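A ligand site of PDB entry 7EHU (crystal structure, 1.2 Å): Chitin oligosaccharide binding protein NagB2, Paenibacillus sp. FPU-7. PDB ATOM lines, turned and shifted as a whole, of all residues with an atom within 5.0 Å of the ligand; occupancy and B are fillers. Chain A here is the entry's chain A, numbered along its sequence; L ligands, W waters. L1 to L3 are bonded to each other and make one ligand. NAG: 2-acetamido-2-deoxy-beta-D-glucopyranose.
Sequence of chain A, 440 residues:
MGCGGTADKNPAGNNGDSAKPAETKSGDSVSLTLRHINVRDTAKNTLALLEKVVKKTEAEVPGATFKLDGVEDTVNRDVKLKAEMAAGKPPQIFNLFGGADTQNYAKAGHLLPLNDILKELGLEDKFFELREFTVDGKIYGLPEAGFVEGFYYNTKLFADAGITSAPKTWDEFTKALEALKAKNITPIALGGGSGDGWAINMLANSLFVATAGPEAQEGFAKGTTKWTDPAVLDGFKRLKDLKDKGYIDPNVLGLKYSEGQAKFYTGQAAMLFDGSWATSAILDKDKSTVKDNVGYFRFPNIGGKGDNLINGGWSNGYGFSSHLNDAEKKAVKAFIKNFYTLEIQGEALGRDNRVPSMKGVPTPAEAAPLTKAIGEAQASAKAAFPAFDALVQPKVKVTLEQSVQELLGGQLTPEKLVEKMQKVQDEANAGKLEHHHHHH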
ATOM      1  N   ILE A  37       7.020 -15.735  15.388  1.00  0.00           N
ATOM      2  CA  ILE A  37       6.397 -15.999  14.096  1.00  0.00           C
ATOM      3  C   ILE A  37       7.418 -16.399  13.030  1.00  0.00           C
ATOM      4  O   ILE A  37       7.087 -16.458  11.841  1.00  0.00           O
ATOM      5  CB  ILE A  37       5.534 -14.809  13.643  1.00  0.00           C
ATOM      6  CG1 ILE A  37       6.369 -13.518  13.523  1.00  0.00           C
ATOM      7  CG2 ILE A  37       4.357 -14.617  14.584  1.00  0.00           C
ATOM      8  CD1 ILE A  37       5.621 -12.416  12.810  1.00  0.00           C
ATOM      9  N   ASN A  38       8.648 -16.708  13.425  1.00  0.00           N
ATOM     10  CA  ASN A  38       9.736 -16.943  12.470  1.00  0.00           C
ATOM     11  C   ASN A  38       9.840 -18.417  12.064  1.00  0.00           C
ATOM     12  O   ASN A  38      10.846 -19.077  12.322  1.00  0.00           O
ATOM     13  CB  ASN A  38      11.039 -16.424  13.045  1.00  0.00           C
ATOM     14  CG  ASN A  38      10.952 -14.965  13.330  1.00  0.00           C
ATOM     15  OD1 ASN A  38      10.594 -14.200  12.427  1.00  0.00           O
ATOM     16  ND2 ASN A  38      11.193 -14.574  14.571  1.00  0.00           N
ATOM     17  N   ARG A  40       8.891 -19.719   8.708  1.00  0.00           N
ATOM     18  CA  ARG A  40       9.131 -20.051   7.314  1.00  0.00           C
ATOM     19  C   ARG A  40      10.623 -20.132   7.021  1.00  0.00           C
ATOM     20  O   ARG A  40      11.454 -19.570   7.743  1.00  0.00           O
ATOM     21  CB  ARG A  40       8.507 -18.997   6.388  1.00  0.00           C
ATOM     22  CG  ARG A  40       6.983 -18.885   6.504  1.00  0.00           C
ATOM     23  CD  ARG A  40       6.437 -17.851   5.484  1.00  0.00           C
ATOM     24  NE  ARG A  40       4.979 -17.657   5.551  1.00  0.00           N
ATOM     25  CZ  ARG A  40       4.343 -16.563   5.975  1.00  0.00           C
ATOM     26  NH1 ARG A  40       4.986 -15.487   6.406  1.00  0.00           N
ATOM     27  NH2 ARG A  40       3.027 -16.541   5.946  1.00  0.00           N
ATOM     28  N   THR A  42      12.300 -18.684   4.811  1.00  0.00           N
ATOM     29  CA  THR A  42      12.865 -17.366   4.551  1.00  0.00           C
ATOM     30  C   THR A  42      13.145 -16.583   5.829  1.00  0.00           C
ATOM     31  O   THR A  42      13.799 -15.542   5.755  1.00  0.00           O
ATOM     32  CB  THR A  42      11.924 -16.554   3.668  1.00  0.00           C
ATOM     33  OG1 THR A  42      10.627 -16.536   4.277  1.00  0.00           O
ATOM     34  CG2 THR A  42      11.816 -17.138   2.253  1.00  0.00           C
ATOM     35  N   ALA A  43      12.632 -17.040   6.971  1.00  0.00           N
ATOM     36  CA  ALA A  43      12.845 -16.386   8.256  1.00  0.00           C
ATOM     37  C   ALA A  43      13.895 -17.081   9.106  1.00  0.00           C
ATOM     38  O   ALA A  43      14.030 -16.748  10.290  1.00  0.00           O
ATOM     39  CB  ALA A  43      11.513 -16.288   9.013  1.00  0.00           C
ATOM     40  N   THR A  46      16.324 -14.851  10.976  1.00  0.00           N
ATOM     41  CA  THR A  46      15.662 -14.163  12.097  1.00  0.00           C
ATOM     42  C   THR A  46      15.522 -15.101  13.275  1.00  0.00           C
ATOM     43  O   THR A  46      15.758 -14.699  14.428  1.00  0.00           O
ATOM     44  CB  THR A  46      14.293 -13.665  11.638  1.00  0.00           C
ATOM     45  OG1 THR A  46      14.462 -12.903  10.438  1.00  0.00           O
ATOM     46  CG2 THR A  46      13.659 -12.760  12.683  1.00  0.00           C
ATOM     47  N   ASP A  73       2.353 -16.439  11.185  1.00  0.00           N
ATOM     48  CA  ASP A  73       1.890 -15.073  11.439  1.00  0.00           C
ATOM     49  C   ASP A  73       0.380 -14.979  11.648  1.00  0.00           C
ATOM     50  O   ASP A  73      -0.084 -14.492  12.701  1.00  0.00           O
ATOM     51  CB  ASP A  73       2.410 -14.116  10.342  1.00  0.00           C
ATOM     52  CG  ASP A  73       2.107 -14.547   8.876  1.00  0.00           C
ATOM     53  OD1 ASP A  73       1.377 -15.510   8.594  1.00  0.00           O
ATOM     54  OD2 ASP A  73       2.681 -13.872   7.976  1.00  0.00           O
ATOM     55  N   THR A  74      -0.416 -15.408  10.669  1.00  0.00           N
ATOM     56  CA  THR A  74      -1.865 -15.211  10.781  1.00  0.00           C
ATOM     57  C   THR A  74      -2.440 -16.029  11.932  1.00  0.00           C
ATOM     58  O   THR A  74      -3.337 -15.567  12.660  1.00  0.00           O
ATOM     59  CB  THR A  74      -2.582 -15.612   9.484  1.00  0.00           C
ATOM     60  OG1 THR A  74      -2.263 -16.962   9.199  1.00  0.00           O
ATOM     61  CG2 THR A  74      -2.208 -14.702   8.318  1.00  0.00           C
ATOM     62  N   ARG A  77      -1.525 -14.258  15.406  1.00  0.00           N
ATOM     63  CA  ARG A  77      -2.191 -13.005  15.706  1.00  0.00           C
ATOM     64  C   ARG A  77      -3.696 -13.170  15.843  1.00  0.00           C
ATOM     65  O   ARG A  77      -4.311 -12.591  16.737  1.00  0.00           O
ATOM     66  CB  ARG A  77      -1.900 -11.984  14.614  1.00  0.00           C
ATOM     67  CG  ARG A  77      -2.403 -10.576  14.907  1.00  0.00           C
ATOM     68  CD  ARG A  77      -2.140  -9.650  13.785  1.00  0.00           C
ATOM     69  NE  ARG A  77      -2.528  -8.307  14.159  1.00  0.00           N
ATOM     70  CZ  ARG A  77      -2.344  -7.234  13.397  1.00  0.00           C
ATOM     71  NH1 ARG A  77      -1.840  -7.395  12.176  1.00  0.00           N
ATOM     72  NH2 ARG A  77      -2.654  -6.022  13.826  1.00  0.00           N
ATOM     73  N   PHE A  97       1.264  -6.989  17.962  1.00  0.00           N
ATOM     74  CA  PHE A  97       1.077  -5.800  17.138  1.00  0.00           C
ATOM     75  C   PHE A  97       0.614  -4.611  17.977  1.00  0.00           C
ATOM     76  O   PHE A  97      -0.244  -4.761  18.855  1.00  0.00           O
ATOM     77  CB  PHE A  97       0.066  -6.056  16.012  1.00  0.00           C
ATOM     78  CG  PHE A  97       0.701  -6.785  14.856  1.00  0.00           C
ATOM     79  CD1 PHE A  97       0.834  -8.171  14.888  1.00  0.00           C
ATOM     80  CD2 PHE A  97       1.255  -6.099  13.781  1.00  0.00           C
ATOM     81  CE1 PHE A  97       1.482  -8.849  13.876  1.00  0.00           C
ATOM     82  CE2 PHE A  97       1.904  -6.761  12.763  1.00  0.00           C
ATOM     83  CZ  PHE A  97       2.031  -8.149  12.803  1.00  0.00           C
ATOM     84  N   GLU A 144      10.305  -4.607  17.067  1.00  0.00           N
ATOM     85  CA  GLU A 144      11.548  -5.278  16.667  1.00  0.00           C
ATOM     86  C   GLU A 144      12.183  -4.612  15.460  1.00  0.00           C
ATOM     87  O   GLU A 144      13.411  -4.640  15.324  1.00  0.00           O
ATOM     88  CB  GLU A 144      11.222  -6.751  16.331  1.00  0.00           C
ATOM     89  CG  GLU A 144      12.320  -7.515  15.665  1.00  0.00           C
ATOM     90  CD  GLU A 144      12.017  -8.974  15.389  1.00  0.00           C
ATOM     91  OE1 GLU A 144      11.058  -9.541  15.946  1.00  0.00           O
ATOM     92  OE2 GLU A 144      12.777  -9.566  14.617  1.00  0.00           O
ATOM     93  N   ALA A 145      11.365  -4.046  14.582  1.00  0.00           N
ATOM     94  CA  ALA A 145      11.808  -3.456  13.340  1.00  0.00           C
ATOM     95  C   ALA A 145      10.803  -2.367  12.993  1.00  0.00           C
ATOM     96  O   ALA A 145       9.722  -2.300  13.568  1.00  0.00           O
ATOM     97  CB  ALA A 145      11.844  -4.492  12.210  1.00  0.00           C
ATOM     98  N   GLY A 146      11.186  -1.516  12.041  1.00  0.00           N
ATOM     99  CA  GLY A 146      10.252  -0.647  11.352  1.00  0.00           C
ATOM    100  C   GLY A 146       9.792  -1.283  10.041  1.00  0.00           C
ATOM    101  O   GLY A 146      10.326  -2.289   9.605  1.00  0.00           O
ATOM    102  N   PHE A 147       8.786  -0.682   9.416  1.00  0.00           N
ATOM    103  CA  PHE A 147       8.359  -1.125   8.101  1.00  0.00           C
ATOM    104  C   PHE A 147       7.856   0.060   7.285  1.00  0.00           C
ATOM    105  O   PHE A 147       7.400   1.071   7.817  1.00  0.00           O
ATOM    106  CB  PHE A 147       7.246  -2.213   8.144  1.00  0.00           C
ATOM    107  CG  PHE A 147       5.857  -1.666   8.381  1.00  0.00           C
ATOM    108  CD1 PHE A 147       5.417  -1.303   9.660  1.00  0.00           C
ATOM    109  CD2 PHE A 147       4.999  -1.478   7.316  1.00  0.00           C
ATOM    110  CE1 PHE A 147       4.160  -0.780   9.853  1.00  0.00           C
ATOM    111  CE2 PHE A 147       3.724  -0.940   7.515  1.00  0.00           C
ATOM    112  CZ  PHE A 147       3.316  -0.578   8.777  1.00  0.00           C
ATOM    113  N   GLU A 149       5.448  -0.097   3.375  1.00  0.00           N
ATOM    114  CA  GLU A 149       4.891  -0.898   2.293  1.00  0.00           C
ATOM    115  C   GLU A 149       4.958  -0.091   1.012  1.00  0.00           C
ATOM    116  O   GLU A 149       4.783   1.121   1.038  1.00  0.00           O
ATOM    117  CB  GLU A 149       3.454  -1.365   2.592  1.00  0.00           C
ATOM    118  CG  GLU A 149       3.392  -2.303   3.799  1.00  0.00           C
ATOM    119  CD  GLU A 149       2.027  -2.826   4.139  1.00  0.00           C
ATOM    120  OE1 GLU A 149       1.068  -2.665   3.326  1.00  0.00           O
ATOM    121  OE2 GLU A 149       1.913  -3.414   5.254  1.00  0.00           O
ATOM    122  N   TRP A 198      -4.911 -10.741   4.345  1.00  0.00           N
ATOM    123  CA  TRP A 198      -4.183  -9.550   4.763  1.00  0.00           C
ATOM    124  C   TRP A 198      -3.220  -9.084   3.672  1.00  0.00           C
ATOM    125  O   TRP A 198      -2.909  -7.887   3.596  1.00  0.00           O
ATOM    126  CB  TRP A 198      -3.419  -9.820   6.065  1.00  0.00           C
ATOM    127  CG  TRP A 198      -2.155 -10.622   5.884  1.00  0.00           C
ATOM    128  CD1 TRP A 198      -2.035 -11.981   5.866  1.00  0.00           C
ATOM    129  CD2 TRP A 198      -0.842 -10.087   5.653  1.00  0.00           C
ATOM    130  NE1 TRP A 198      -0.727 -12.323   5.638  1.00  0.00           N
ATOM    131  CE2 TRP A 198       0.021 -11.187   5.499  1.00  0.00           C
ATOM    132  CE3 TRP A 198      -0.316  -8.783   5.551  1.00  0.00           C
ATOM    133  CZ2 TRP A 198       1.382 -11.020   5.313  1.00  0.00           C
ATOM    134  CZ3 TRP A 198       1.024  -8.641   5.341  1.00  0.00           C
ATOM    135  CH2 TRP A 198       1.858  -9.749   5.215  1.00  0.00           C
ATOM    136  N   TYR A 257       0.534 -16.211   0.681  1.00  0.00           N
ATOM    137  CA  TYR A 257       1.348 -15.000   0.693  1.00  0.00           C
ATOM    138  C   TYR A 257       2.748 -15.266   0.163  1.00  0.00           C
ATOM    139  O   TYR A 257       3.226 -14.544  -0.709  1.00  0.00           O
ATOM    140  CB  TYR A 257       1.445 -14.501   2.145  1.00  0.00           C
ATOM    141  CG  TYR A 257       2.372 -13.353   2.391  1.00  0.00           C
ATOM    142  CD1 TYR A 257       2.268 -12.175   1.685  1.00  0.00           C
ATOM    143  CD2 TYR A 257       3.344 -13.451   3.367  1.00  0.00           C
ATOM    144  CE1 TYR A 257       3.120 -11.114   1.936  1.00  0.00           C
ATOM    145  CE2 TYR A 257       4.192 -12.417   3.642  1.00  0.00           C
ATOM    146  CZ  TYR A 257       4.067 -11.232   2.937  1.00  0.00           C
ATOM    147  OH  TYR A 257       4.918 -10.198   3.266  1.00  0.00           O
ATOM    148  N   GLN A 261       5.033 -13.923  -3.148  1.00  0.00           N
ATOM    149  CA  GLN A 261       6.379 -13.366  -3.092  1.00  0.00           C
ATOM    150  C   GLN A 261       7.302 -14.108  -4.063  1.00  0.00           C
ATOM    151  O   GLN A 261       8.063 -13.469  -4.795  1.00  0.00           O
ATOM    152  CB  GLN A 261       6.927 -13.463  -1.670  1.00  0.00           C
ATOM    153  CG  GLN A 261       6.207 -12.565  -0.676  1.00  0.00           C
ATOM    154  CD  GLN A 261       6.746 -12.723   0.729  1.00  0.00           C
ATOM    155  OE1 GLN A 261       7.083 -13.845   1.133  1.00  0.00           O
ATOM    156  NE2 GLN A 261       6.879 -11.622   1.451  1.00  0.00           N
ATOM    157  N   TRP A 277       9.944  -5.942   5.239  1.00  0.00           N
ATOM    158  CA  TRP A 277      10.419  -7.207   5.812  1.00  0.00           C
ATOM    159  C   TRP A 277      10.551  -8.304   4.752  1.00  0.00           C
ATOM    160  O   TRP A 277      11.097  -9.363   5.070  1.00  0.00           O
ATOM    161  CB  TRP A 277       9.446  -7.651   6.932  1.00  0.00           C
ATOM    162  CG  TRP A 277       8.064  -7.920   6.373  1.00  0.00           C
ATOM    163  CD1 TRP A 277       7.673  -8.990   5.609  1.00  0.00           C
ATOM    164  CD2 TRP A 277       6.916  -7.049   6.456  1.00  0.00           C
ATOM    165  NE1 TRP A 277       6.371  -8.847   5.202  1.00  0.00           N
ATOM    166  CE2 TRP A 277       5.885  -7.669   5.713  1.00  0.00           C
ATOM    167  CE3 TRP A 277       6.667  -5.831   7.084  1.00  0.00           C
ATOM    168  CZ2 TRP A 277       4.627  -7.075   5.574  1.00  0.00           C
ATOM    169  CZ3 TRP A 277       5.428  -5.261   6.950  1.00  0.00           C
ATOM    170  CH2 TRP A 277       4.419  -5.889   6.206  1.00  0.00           C
ATOM    171  N   ALA A 278      10.127  -8.041   3.520  1.00  0.00           N
ATOM    172  CA  ALA A 278      10.264  -9.003   2.425  1.00  0.00           C
ATOM    173  C   ALA A 278      11.605  -8.902   1.726  1.00  0.00           C
ATOM    174  O   ALA A 278      11.925  -9.756   0.890  1.00  0.00           O
ATOM    175  CB  ALA A 278       9.157  -8.767   1.383  1.00  0.00           C
ATOM    176  N   SER A 280      14.743  -9.477   2.304  1.00  0.00           N
ATOM    177  CA  SER A 280      15.707 -10.575   2.312  1.00  0.00           C
ATOM    178  C   SER A 280      15.318 -11.655   1.316  1.00  0.00           C
ATOM    179  O   SER A 280      16.183 -12.270   0.685  1.00  0.00           O
ATOM    180  CB  SER A 280      15.848 -11.199   3.706  1.00  0.00           C
ATOM    181  OG  SER A 280      14.593 -11.651   4.176  1.00  0.00           O
ATOM    182  N   ALA A 281      14.014 -11.944   1.175  1.00  0.00           N
ATOM    183  CA  ALA A 281      13.600 -12.973   0.232  1.00  0.00           C
ATOM    184  C   ALA A 281      13.868 -12.527  -1.201  1.00  0.00           C
ATOM    185  O   ALA A 281      14.203 -13.351  -2.052  1.00  0.00           O
ATOM    186  CB  ALA A 281      12.125 -13.294   0.433  1.00  0.00           C
ATOM    187  N   SER A 315       5.362  -1.237  14.217  1.00  0.00           N
ATOM    188  CA  SER A 315       4.113  -1.876  14.582  1.00  0.00           C
ATOM    189  C   SER A 315       4.251  -3.256  15.208  1.00  0.00           C
ATOM    190  O   SER A 315       3.263  -3.735  15.765  1.00  0.00           O
ATOM    191  CB  SER A 315       3.280  -2.078  13.306  1.00  0.00           C
ATOM    192  OG  SER A 315       4.031  -2.880  12.396  1.00  0.00           O
ATOM    193  N   ASN A 316       5.376  -3.937  15.067  1.00  0.00           N
ATOM    194  CA  ASN A 316       5.448  -5.354  15.428  1.00  0.00           C
ATOM    195  C   ASN A 316       6.710  -5.634  16.216  1.00  0.00           C
ATOM    196  O   ASN A 316       7.807  -5.198  15.846  1.00  0.00           O
ATOM    197  CB  ASN A 316       5.386  -6.223  14.166  1.00  0.00           C
ATOM    198  CG  ASN A 316       5.276  -7.709  14.476  1.00  0.00           C
ATOM    199  OD1 ASN A 316       6.107  -8.505  14.020  1.00  0.00           O
ATOM    200  ND2 ASN A 316       4.270  -8.093  15.261  1.00  0.00           N
ATOM    201  N   ASP A 352      19.933  -9.466   6.901  1.00  0.00           N
ATOM    202  CA  ASP A 352      18.596  -9.672   6.372  1.00  0.00           C
ATOM    203  C   ASP A 352      17.950  -8.390   5.954  1.00  0.00           C
ATOM    204  O   ASP A 352      16.751  -8.403   5.622  1.00  0.00           O
ATOM    205  CB  ASP A 352      17.701 -10.351   7.378  1.00  0.00           C
ATOM    206  CG  ASP A 352      17.646 -11.793   7.154  1.00  0.00           C
ATOM    207  OD1 ASP A 352      18.281 -12.295   6.189  1.00  0.00           O
ATOM    208  OD2 ASP A 352      16.877 -12.393   7.908  1.00  0.00           O
ATOM    209  N   ARG A 354      16.922  -6.142   7.625  1.00  0.00           N
ATOM    210  CA  ARG A 354      15.821  -5.844   8.532  1.00  0.00           C
ATOM    211  C   ARG A 354      15.986  -4.413   9.084  1.00  0.00           C
ATOM    212  O   ARG A 354      17.061  -4.032   9.549  1.00  0.00           O
ATOM    213  CB  ARG A 354      15.708  -6.905   9.630  1.00  0.00           C
ATOM    214  CG  ARG A 354      15.599  -8.382   9.112  1.00  0.00           C
ATOM    215  CD  ARG A 354      14.735  -9.369   9.970  1.00  0.00           C
ATOM    216  NE  ARG A 354      15.401  -9.705  11.241  1.00  0.00           N
ATOM    217  CZ  ARG A 354      16.401 -10.582  11.372  1.00  0.00           C
ATOM    218  NH1 ARG A 354      16.908 -11.254  10.341  1.00  0.00           N
ATOM    219  NH2 ARG A 354      16.940 -10.762  12.563  1.00  0.00           N
ATOM    220  N   ALA A 387      -0.672   1.092   9.242  1.00  0.00           N
ATOM    221  CA  ALA A 387      -1.585   0.120   8.650  1.00  0.00           C
ATOM    222  C   ALA A 387      -2.957   0.227   9.306  1.00  0.00           C
ATOM    223  O   ALA A 387      -3.085   0.489  10.508  1.00  0.00           O
ATOM    224  CB  ALA A 387      -1.047  -1.295   8.801  1.00  0.00           C
ATOM    225  N   ASP A 389      -4.915  -1.903  10.314  1.00  0.00           N
ATOM    226  CA  ASP A 389      -5.156  -2.854  11.404  1.00  0.00           C
ATOM    227  C   ASP A 389      -4.571  -2.388  12.723  1.00  0.00           C
ATOM    228  O   ASP A 389      -4.897  -2.970  13.768  1.00  0.00           O
ATOM    229  CB  ASP A 389      -4.729  -4.196  10.852  1.00  0.00           C
ATOM    230  CG  ASP A 389      -3.233  -4.475  10.831  1.00  0.00           C
ATOM    231  OD1 ASP A 389      -2.315  -4.178  11.460  1.00  0.00           O
ATOM    232  OD2 ASP A 389      -2.952  -4.080   9.618  1.00  0.00           O
HETATM  233  C1  NAG L   1      11.607 -11.954   8.486  1.00  0.00           C
HETATM  234  C2  NAG L   1      10.350 -12.284   7.658  1.00  0.00           C
HETATM  235  C3  NAG L   1       9.236 -11.287   7.929  1.00  0.00           C
HETATM  236  C4  NAG L   1       9.083 -10.992   9.420  1.00  0.00           C
HETATM  237  C5  NAG L   1      10.430 -10.781  10.086  1.00  0.00           C
HETATM  238  C6  NAG L   1      10.343 -10.630  11.582  1.00  0.00           C
HETATM  239  C7  NAG L   1      10.685 -13.304   5.412  1.00  0.00           C
HETATM  240  C8  NAG L   1      11.077 -13.028   3.988  1.00  0.00           C
HETATM  241  N2  NAG L   1      10.684 -12.256   6.239  1.00  0.00           N
HETATM  242  O1  NAG L   1      12.571 -12.936   8.321  1.00  0.00           O
HETATM  243  O3  NAG L   1       8.026 -11.797   7.359  1.00  0.00           O
HETATM  244  O4  NAG L   1       8.428  -9.728   9.565  1.00  0.00           O
HETATM  245  O5  NAG L   1      11.278 -11.894   9.828  1.00  0.00           O
HETATM  246  O6  NAG L   1       9.535 -11.633  12.165  1.00  0.00           O
HETATM  247  O7  NAG L   1      10.366 -14.428   5.804  1.00  0.00           O
HETATM  248  C1  NAG L   2       7.047  -9.715   9.910  1.00  0.00           C
HETATM  249  C2  NAG L   2       6.758  -8.288  10.309  1.00  0.00           C
HETATM  250  C3  NAG L   2       5.250  -8.066  10.478  1.00  0.00           C
HETATM  251  C4  NAG L   2       4.464  -8.606   9.298  1.00  0.00           C
HETATM  252  C5  NAG L   2       4.898 -10.050   9.044  1.00  0.00           C
HETATM  253  C6  NAG L   2       4.240 -10.695   7.848  1.00  0.00           C
HETATM  254  C7  NAG L   2       8.567  -7.241  11.647  1.00  0.00           C
HETATM  255  C8  NAG L   2       9.112  -7.069  13.029  1.00  0.00           C
HETATM  256  N2  NAG L   2       7.435  -7.960  11.550  1.00  0.00           N
HETATM  257  O3  NAG L   2       5.044  -6.676  10.654  1.00  0.00           O
HETATM  258  O4  NAG L   2       3.076  -8.621   9.614  1.00  0.00           O
HETATM  259  O5  NAG L   2       6.300 -10.069   8.789  1.00  0.00           O
HETATM  260  O6  NAG L   2       4.616 -12.059   7.738  1.00  0.00           O
HETATM  261  O7  NAG L   2       9.110  -6.753  10.666  1.00  0.00           O
HETATM  262  C1  NAG L   3       2.243  -7.728   8.941  1.00  0.00           C
HETATM  263  C2  NAG L   3       0.822  -8.050   9.319  1.00  0.00           C
HETATM  264  C3  NAG L   3      -0.139  -6.991   8.761  1.00  0.00           C
HETATM  265  C4  NAG L   3       0.306  -5.599   9.200  1.00  0.00           C
HETATM  266  C5  NAG L   3       1.768  -5.362   8.830  1.00  0.00           C
HETATM  267  C6  NAG L   3       2.309  -4.042   9.321  1.00  0.00           C
HETATM  268  C7  NAG L   3       0.153 -10.375   9.720  1.00  0.00           C
HETATM  269  C8  NAG L   3      -0.261 -11.669   9.097  1.00  0.00           C
HETATM  270  N2  NAG L   3       0.426  -9.373   8.877  1.00  0.00           N
HETATM  271  O3  NAG L   3      -1.446  -7.290   9.241  1.00  0.00           O
HETATM  272  O4  NAG L   3      -0.462  -4.578   8.583  1.00  0.00           O
HETATM  273  O5  NAG L   3       2.574  -6.411   9.373  1.00  0.00           O
HETATM  274  O6  NAG L   3       2.248  -3.939  10.739  1.00  0.00           O
HETATM  275  O7  NAG L   3       0.225 -10.221  10.944  1.00  0.00           O
HETATM  276  O   HOH W   1      15.530 -14.551   7.963  1.00  0.00           O
HETATM  277  O   HOH W   2       7.783 -12.262   4.411  1.00  0.00           O
HETATM  278  O   HOH W   3      -3.057  -9.400  10.257  1.00  0.00           O
HETATM  279  O   HOH W   4      -3.523  -6.183   7.870  1.00  0.00           O
HETATM  280  O   HOH W   5      -0.562  -4.145   5.915  1.00  0.00           O
HETATM  281  O   HOH W   6       7.055  -4.611  10.618  1.00  0.00           O
HETATM  282  O   HOH W   7      11.817  -7.327  10.085  1.00  0.00           O
HETATM  283  O   HOH W   8       6.189 -13.694   9.425  1.00  0.00           O
HETATM  284  O   HOH W   9       9.654 -11.573  14.806  1.00  0.00           O
HETATM  285  O   HOH W  10       7.866 -15.197   6.971  1.00  0.00           O
HETATM  286  O   HOH W  11       8.829 -14.369  10.039  1.00  0.00           O
HETATM  287  O   HOH W  12      14.493 -11.504   6.839  1.00  0.00           O
HETATM  288  O   HOH W  13       1.267 -12.024  12.808  1.00  0.00           O
HETATM  289  O   HOH W  14      -0.002  -2.885  11.786  1.00  0.00           O
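OD2 of Asp 73 lies within salt-bridge range of NH1 of Arg 40, 3.2 Å away.
The side-chain carboxylate (OD1) of Asp 389 is in salt-bridge range of the guanidinium group (NH2) of Arg 77 (3.0 Å).
OG1 of Thr 46 sits at hydrogen-bond distance from NH1 of Arg 354, at 3.0 Å.
N of Glu 144 is in hydrogen-bond range of O of Asn 316.
The indole nitrogen (NE1) of Trp 277 is in hydrogen-bond range of the side-chain hydroxyl (OH) of Tyr 257.
Water W9 lies within hydrogen-bond range of O6 of NAG L1 (2.6 Å), OE1 of Glu 144 (2.7 Å) and ND2 of Asn 38 (3.4 Å).
Water W14 lies within hydrogen-bond range of OD1 of Asp 389 (2.7 Å) and O6 of NAG L3 (2.7 Å).
Water W5 bridges the side-chain carboxylate (OE2) of Glu 149 (2.7 Å) and an oxygen (O4) of NAG L3 (2.7 Å).
Water W13 bridges an oxygen (O7) of NAG L3 (2.8 Å) and the backbone carbonyl oxygen of Asp 73 (2.8 Å).
Water W12 lies within hydrogen-bond range of OG of Ser 280 (2.7 Å), OD2 of Asp 352 (2.8 Å) and O1 of NAG L1 (2.8 Å).
Water W10 bridges O7 of NAG L1 (2.9 Å) and NH1 of Arg 40 (2.9 Å).
OG1 of Thr 42 sits at hydrogen-bond distance from O7 of NAG L1, 2.6 Å away.
The side-chain hydroxyl (OG) of Ser 315 sits at hydrogen-bond distance from an oxygen (O6) of NAG L3, at 2.7 Å.
OD2 of Asp 73 lies within hydrogen-bond range of O6 of NAG L2 (2.7 Å).
The side-chain carboxylate (OD2) of Asp 389 is in hydrogen-bond range of an oxygen (O4) of NAG L3 (2.7 Å).
An oxygen (O6) of NAG L1 is in hydrogen-bond range of the side-chain amide oxygen (OD1) of Asn 38 (2.8 Å).
The side-chain hydroxyl (OG1) of Thr 46 is in hydrogen-bond range of an oxygen (O1) of NAG L1, at 2.8 Å.
The side-chain amide oxygen (OD1) of Asn 316 lies within hydrogen-bond range of a nitrogen (N2) of NAG L2 (2.9 Å).
The guanidinium group of Arg 77 is in hydrogen-bond range of an oxygen (O3) of NAG L3, at 3.0 Å.
O of Trp 277 is in hydrogen-bond range of N2 of NAG L1, at 3.1 Å.
CG1 of Ile 37 touches O6 of NAG L1, 3.9 Å away.
NH1 of Arg 40 touches O6 of NAG L2 (3.7 Å).
CA of Ala 43 touches O1 of NAG L1, at 3.5 Å.
Thr 74 touches the ligand.
CZ of Phe 97 touches O7 of NAG L3, at 3.3 Å.
Glu 144 touches the ligand.
CB of Ala 145 touches C8 of NAG L2 (3.8 Å).
Phe 147 touches the ligand.
CE3 of Trp 198 touches N2 of NAG L3 (3.5 Å).
OG of Ser 280 touches C8 of NAG L1 (3.8 Å).
CB of Ala 281 touches C8 of NAG L1 (3.7 Å).
CB of Ala 387 touches O4 of NAG L3 (3.3 Å).
Hydrophobic or aromatic side chains that line the ligand: Ile 37, Ala 43, Phe 97, Ala 145, Phe 147, Trp 198, Trp 277, Ala 281 and Ala 387.
Of the 28 residues printed, 21 come within 4 Å of the ligand.
Along chain A the residues within 4 Å of the ligand span positions 37 to 389.
The nearest printed residue that does not touch the ligand is Glu 149 (4.1 Å).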
